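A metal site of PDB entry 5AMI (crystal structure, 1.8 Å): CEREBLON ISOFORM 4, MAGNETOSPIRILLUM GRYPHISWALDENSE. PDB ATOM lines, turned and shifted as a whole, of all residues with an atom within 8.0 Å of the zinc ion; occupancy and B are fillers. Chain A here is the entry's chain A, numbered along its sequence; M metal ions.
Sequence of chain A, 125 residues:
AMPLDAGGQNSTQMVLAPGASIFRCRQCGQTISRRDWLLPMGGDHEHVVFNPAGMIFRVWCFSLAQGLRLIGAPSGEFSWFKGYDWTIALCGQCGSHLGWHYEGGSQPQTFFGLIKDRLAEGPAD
The backbone NH (N) of Cys 25 is in hydrogen-bond range of the backbone carbonyl oxygen (O) of Gln 30 (2.9 Å). The side-chain sulfur (SG) of Cys 94 sits close to the backbone NH (N) of Ser 96. N of Cys 91 lies within hydrogen-bond range of O of Ser 96 (2.7 Å). SG of Cys 91 lies close to N of Gln 93. The side-chain sulfur (SG) of Cys 25 lies close to the backbone NH (N) of Gln 27, 3.4 Å away. The side-chain amide nitrogen (NE2) of Gln 93 lies close to the side-chain sulfur (SG) of Cys 28, 3.2 Å away. The backbone NH (N) of Gln 30 lies close to the side-chain sulfur (SG) of Cys 28, 3.5 Å away.
The zinc ion is bound by the side-chain sulfur of Cys 91 (2.3 Å), the side-chain sulfur of Cys 25 (2.3 Å), the side-chain sulfur of Cys 94 (2.3 Å) and the side-chain sulfur of Cys 28 (2.4 Å).
Within 4 Å of the zinc ion: Cys 25, Cys 28, Cys 91 and Cys 94.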
ATOM      1  N   ARG A  24     -16.709 -24.629  27.885  1.00  0.00           N
ATOM      2  CA  ARG A  24     -16.539 -25.796  26.994  1.00  0.00           C
ATOM      3  C   ARG A  24     -16.165 -25.370  25.598  1.00  0.00           C
ATOM      4  O   ARG A  24     -16.321 -24.198  25.213  1.00  0.00           O
ATOM      5  CB  ARG A  24     -17.873 -26.581  26.897  1.00  0.00           C
ATOM      6  CG  ARG A  24     -18.282 -27.276  28.186  1.00  0.00           C
ATOM      7  CD  ARG A  24     -19.587 -28.052  28.047  1.00  0.00           C
ATOM      8  NE  ARG A  24     -19.822 -28.709  29.307  1.00  0.00           N
ATOM      9  CZ  ARG A  24     -19.145 -29.746  29.765  1.00  0.00           C
ATOM     10  NH1 ARG A  24     -18.275 -30.414  29.007  1.00  0.00           N
ATOM     11  NH2 ARG A  24     -19.346 -30.135  31.011  1.00  0.00           N
ATOM     12  N   CYS A  25     -15.538 -26.268  24.829  1.00  0.00           N
ATOM     13  CA  CYS A  25     -15.242 -25.986  23.443  1.00  0.00           C
ATOM     14  C   CYS A  25     -16.565 -25.781  22.696  1.00  0.00           C
ATOM     15  O   CYS A  25     -17.454 -26.629  22.752  1.00  0.00           O
ATOM     16  CB  CYS A  25     -14.457 -27.213  22.778  1.00  0.00           C
ATOM     17  SG  CYS A  25     -14.183 -27.018  21.002  1.00  0.00           S
ATOM     18  N   ARG A  26     -16.659 -24.693  21.959  1.00  0.00           N
ATOM     19  CA  ARG A  26     -17.867 -24.380  21.267  1.00  0.00           C
ATOM     20  C   ARG A  26     -18.173 -25.366  20.146  1.00  0.00           C
ATOM     21  O   ARG A  26     -19.322 -25.538  19.748  1.00  0.00           O
ATOM     22  CB  ARG A  26     -17.725 -22.983  20.740  1.00  0.00           C
ATOM     23  CG  ARG A  26     -18.821 -22.531  19.851  1.00  0.00           C
ATOM     24  CD  ARG A  26     -18.562 -21.094  19.359  1.00  0.00           C
ATOM     25  NE  ARG A  26     -19.609 -20.741  18.436  1.00  0.00           N
ATOM     26  CZ  ARG A  26     -19.710 -19.552  17.805  1.00  0.00           C
ATOM     27  NH1 ARG A  26     -18.818 -18.607  18.005  1.00  0.00           N
ATOM     28  NH2 ARG A  26     -20.657 -19.363  16.976  1.00  0.00           N
ATOM     29  N   GLN A  27     -17.104 -25.937  19.574  1.00  0.00           N
ATOM     30  CA  GLN A  27     -17.229 -26.820  18.396  1.00  0.00           C
ATOM     31  C   GLN A  27     -17.619 -28.240  18.741  1.00  0.00           C
ATOM     32  O   GLN A  27     -18.298 -28.900  17.930  1.00  0.00           O
ATOM     33  CB  GLN A  27     -15.926 -26.806  17.598  1.00  0.00           C
ATOM     34  CG  GLN A  27     -15.630 -25.479  16.942  1.00  0.00           C
ATOM     35  CD  GLN A  27     -16.830 -24.905  16.178  1.00  0.00           C
ATOM     36  OE1 GLN A  27     -17.338 -23.828  16.505  1.00  0.00           O
ATOM     37  NE2 GLN A  27     -17.344 -25.659  15.217  1.00  0.00           N
ATOM     38  N   CYS A  28     -17.327 -28.708  19.954  1.00  0.00           N
ATOM     39  CA  CYS A  28     -17.681 -30.076  20.290  1.00  0.00           C
ATOM     40  C   CYS A  28     -18.138 -30.364  21.710  1.00  0.00           C
ATOM     41  O   CYS A  28     -18.689 -31.419  21.973  1.00  0.00           O
ATOM     42  CB  CYS A  28     -16.485 -30.991  20.006  1.00  0.00           C
ATOM     43  SG  CYS A  28     -15.156 -30.805  21.243  1.00  0.00           S
ATOM     44  N   GLY A  29     -17.996 -29.405  22.641  1.00  0.00           N
ATOM     45  CA  GLY A  29     -18.402 -29.587  23.995  1.00  0.00           C
ATOM     46  C   GLY A  29     -17.402 -30.048  24.993  1.00  0.00           C
ATOM     47  O   GLY A  29     -17.712 -30.168  26.177  1.00  0.00           O
ATOM     48  N   GLN A  30     -16.182 -30.344  24.566  1.00  0.00           N
ATOM     49  CA  GLN A  30     -15.092 -30.699  25.485  1.00  0.00           C
ATOM     50  C   GLN A  30     -15.014 -29.744  26.679  1.00  0.00           C
ATOM     51  O   GLN A  30     -15.038 -28.540  26.486  1.00  0.00           O
ATOM     52  CB  GLN A  30     -13.743 -30.616  24.723  1.00  0.00           C
ATOM     53  CG  GLN A  30     -12.490 -30.905  25.559  1.00  0.00           C
ATOM     54  CD  GLN A  30     -12.219 -32.388  25.685  1.00  0.00           C
ATOM     55  OE1 GLN A  30     -13.117 -33.147  25.945  1.00  0.00           O
ATOM     56  NE2 GLN A  30     -10.940 -32.812  25.541  1.00  0.00           N
ATOM     57  N   THR A  31     -14.898 -30.274  27.894  1.00  0.00           N
ATOM     58  CA  THR A  31     -14.725 -29.457  29.070  1.00  0.00           C
ATOM     59  C   THR A  31     -13.316 -28.812  29.080  1.00  0.00           C
ATOM     60  O   THR A  31     -12.342 -29.527  28.952  1.00  0.00           O
ATOM     61  CB  THR A  31     -14.808 -30.326  30.371  1.00  0.00           C
ATOM     62  OG1 THR A  31     -15.926 -31.245  30.269  1.00  0.00           O
ATOM     63  CG2 THR A  31     -15.048 -29.379  31.532  1.00  0.00           C
ATOM     64  N   ILE A  32     -13.250 -27.498  29.270  1.00  0.00           N
ATOM     65  CA  ILE A  32     -12.002 -26.712  29.102  1.00  0.00           C
ATOM     66  C   ILE A  32     -11.642 -25.940  30.408  1.00  0.00           C
ATOM     67  O   ILE A  32     -10.535 -26.084  30.898  1.00  0.00           O
ATOM     68  CB  ILE A  32     -12.013 -25.745  27.940  1.00  0.00           C
ATOM     69  CG1 ILE A  32     -12.250 -26.446  26.643  1.00  0.00           C
ATOM     70  CG2 ILE A  32     -10.736 -24.924  27.870  1.00  0.00           C
ATOM     71  CD1 ILE A  32     -11.269 -27.466  26.219  1.00  0.00           C
ATOM     72  N   GLY A  67      -8.338 -30.447  29.010  1.00  0.00           N
ATOM     73  CA  GLY A  67      -8.990 -30.920  27.782  1.00  0.00           C
ATOM     74  C   GLY A  67      -8.381 -30.382  26.487  1.00  0.00           C
ATOM     75  O   GLY A  67      -8.991 -30.474  25.416  1.00  0.00           O
ATOM     76  N   LEU A  68      -7.209 -29.737  26.603  1.00  0.00           N
ATOM     77  CA  LEU A  68      -6.527 -29.128  25.479  1.00  0.00           C
ATOM     78  C   LEU A  68      -5.483 -30.086  24.995  1.00  0.00           C
ATOM     79  O   LEU A  68      -5.151 -31.014  25.660  1.00  0.00           O
ATOM     80  CB  LEU A  68      -5.884 -27.783  25.923  1.00  0.00           C
ATOM     81  CG  LEU A  68      -6.925 -26.713  26.294  1.00  0.00           C
ATOM     82  CD1 LEU A  68      -6.212 -25.599  27.077  1.00  0.00           C
ATOM     83  CD2 LEU A  68      -7.711 -26.214  25.067  1.00  0.00           C
ATOM     84  N   LEU A  90      -4.914 -26.446  21.170  1.00  0.00           N
ATOM     85  CA  LEU A  90      -6.041 -27.027  20.474  1.00  0.00           C
ATOM     86  C   LEU A  90      -6.985 -27.670  21.474  1.00  0.00           C
ATOM     87  O   LEU A  90      -6.554 -28.162  22.511  1.00  0.00           O
ATOM     88  CB  LEU A  90      -5.628 -28.104  19.467  1.00  0.00           C
ATOM     89  CG  LEU A  90      -4.592 -27.598  18.441  1.00  0.00           C
ATOM     90  CD1 LEU A  90      -4.364 -28.670  17.424  1.00  0.00           C
ATOM     91  CD2 LEU A  90      -4.988 -26.288  17.784  1.00  0.00           C
ATOM     92  N   CYS A  91      -8.250 -27.715  21.086  1.00  0.00           N
ATOM     93  CA  CYS A  91      -9.185 -28.629  21.788  1.00  0.00           C
ATOM     94  C   CYS A  91      -8.629 -30.052  21.654  1.00  0.00           C
ATOM     95  O   CYS A  91      -8.333 -30.511  20.532  1.00  0.00           O
ATOM     96  CB  CYS A  91     -10.610 -28.491  21.190  1.00  0.00           C
ATOM     97  SG  CYS A  91     -11.758 -29.740  21.895  1.00  0.00           S
ATOM     98  N   GLY A  92      -8.450 -30.780  22.758  1.00  0.00           N
ATOM     99  CA  GLY A  92      -7.906 -32.122  22.728  1.00  0.00           C
ATOM    100  C   GLY A  92      -8.841 -33.154  22.069  1.00  0.00           C
ATOM    101  O   GLY A  92      -8.420 -34.245  21.648  1.00  0.00           O
ATOM    102  N   GLN A  93     -10.111 -32.802  21.992  1.00  0.00           N
ATOM    103  CA  GLN A  93     -11.119 -33.697  21.430  1.00  0.00           C
ATOM    104  C   GLN A  93     -11.275 -33.442  19.933  1.00  0.00           C
ATOM    105  O   GLN A  93     -11.144 -34.401  19.169  1.00  0.00           O
ATOM    106  CB  GLN A  93     -12.421 -33.514  22.184  1.00  0.00           C
ATOM    107  CG  GLN A  93     -13.555 -34.423  21.728  1.00  0.00           C
ATOM    108  CD  GLN A  93     -14.627 -34.534  22.801  1.00  0.00           C
ATOM    109  OE1 GLN A  93     -14.644 -35.475  23.586  1.00  0.00           O
ATOM    110  NE2 GLN A  93     -15.539 -33.567  22.813  1.00  0.00           N
ATOM    111  N   CYS A  94     -11.575 -32.214  19.504  1.00  0.00           N
ATOM    112  CA  CYS A  94     -11.879 -31.932  18.078  1.00  0.00           C
ATOM    113  C   CYS A  94     -10.767 -31.266  17.278  1.00  0.00           C
ATOM    114  O   CYS A  94     -10.887 -31.233  16.046  1.00  0.00           O
ATOM    115  CB  CYS A  94     -13.183 -31.170  17.875  1.00  0.00           C
ATOM    116  SG  CYS A  94     -13.047 -29.387  18.292  1.00  0.00           S
ATOM    117  N   GLY A  95      -9.722 -30.816  17.944  1.00  0.00           N
ATOM    118  CA  GLY A  95      -8.624 -30.070  17.281  1.00  0.00           C
ATOM    119  C   GLY A  95      -8.877 -28.616  16.965  1.00  0.00           C
ATOM    120  O   GLY A  95      -7.977 -27.964  16.389  1.00  0.00           O
ATOM    121  N   SER A  96     -10.010 -28.046  17.383  1.00  0.00           N
ATOM    122  CA  SER A  96     -10.268 -26.580  17.248  1.00  0.00           C
ATOM    123  C   SER A  96      -9.187 -25.772  17.913  1.00  0.00           C
ATOM    124  O   SER A  96      -8.751 -26.111  19.035  1.00  0.00           O
ATOM    125  CB  SER A  96     -11.658 -26.189  17.882  1.00  0.00           C
ATOM    126  OG  SER A  96     -11.980 -24.798  17.716  1.00  0.00           O
ATOM    127  N   HIS A  97      -8.746 -24.695  17.279  1.00  0.00           N
ATOM    128  CA  HIS A  97      -7.789 -23.831  17.938  1.00  0.00           C
ATOM    129  C   HIS A  97      -8.467 -22.920  18.992  1.00  0.00           C
ATOM    130  O   HIS A  97      -9.252 -22.089  18.647  1.00  0.00           O
ATOM    131  CB  HIS A  97      -7.038 -23.025  16.899  1.00  0.00           C
ATOM    132  CG  HIS A  97      -6.094 -22.082  17.508  1.00  0.00           C
ATOM    133  ND1 HIS A  97      -5.766 -20.897  16.911  1.00  0.00           N
ATOM    134  CD2 HIS A  97      -5.378 -22.157  18.649  1.00  0.00           C
ATOM    135  CE1 HIS A  97      -4.853 -20.271  17.651  1.00  0.00           C
ATOM    136  NE2 HIS A  97      -4.629 -20.993  18.730  1.00  0.00           N
ATOM    137  N   LEU A  98      -8.229 -23.178  20.284  1.00  0.00           N
ATOM    138  CA  LEU A  98      -8.899 -22.494  21.349  1.00  0.00           C
ATOM    139  C   LEU A  98      -8.076 -21.344  21.949  1.00  0.00           C
ATOM    140  O   LEU A  98      -8.622 -20.496  22.653  1.00  0.00           O
ATOM    141  CB  LEU A  98      -9.327 -23.434  22.499  1.00  0.00           C
ATOM    142  CG  LEU A  98     -10.355 -24.498  22.050  1.00  0.00           C
ATOM    143  CD1 LEU A  98     -10.825 -25.302  23.254  1.00  0.00           C
ATOM    144  CD2 LEU A  98     -11.488 -23.950  21.234  1.00  0.00           C
ATOM    145  N   ARG A 118     -14.531 -18.811  20.983  1.00  0.00           N
ATOM    146  CA  ARG A 118     -14.364 -20.246  20.632  1.00  0.00           C
ATOM    147  C   ARG A 118     -14.791 -21.169  21.765  1.00  0.00           C
ATOM    148  O   ARG A 118     -14.659 -22.371  21.657  1.00  0.00           O
ATOM    149  CB  ARG A 118     -12.934 -20.517  20.138  1.00  0.00           C
ATOM    150  CG  ARG A 118     -12.706 -19.803  18.830  1.00  0.00           C
ATOM    151  CD  ARG A 118     -11.401 -20.045  18.223  1.00  0.00           C
ATOM    152  NE  ARG A 118     -11.185 -19.069  17.114  1.00  0.00           N
ATOM    153  CZ  ARG A 118     -10.125 -19.125  16.339  1.00  0.00           C
ATOM    154  NH1 ARG A 118      -9.231 -20.057  16.563  1.00  0.00           N
ATOM    155  NH2 ARG A 118      -9.942 -18.227  15.384  1.00  0.00           N
HETATM  156 ZN    ZN M   1     -13.557 -29.202  20.565  1.00  0.00          ZN
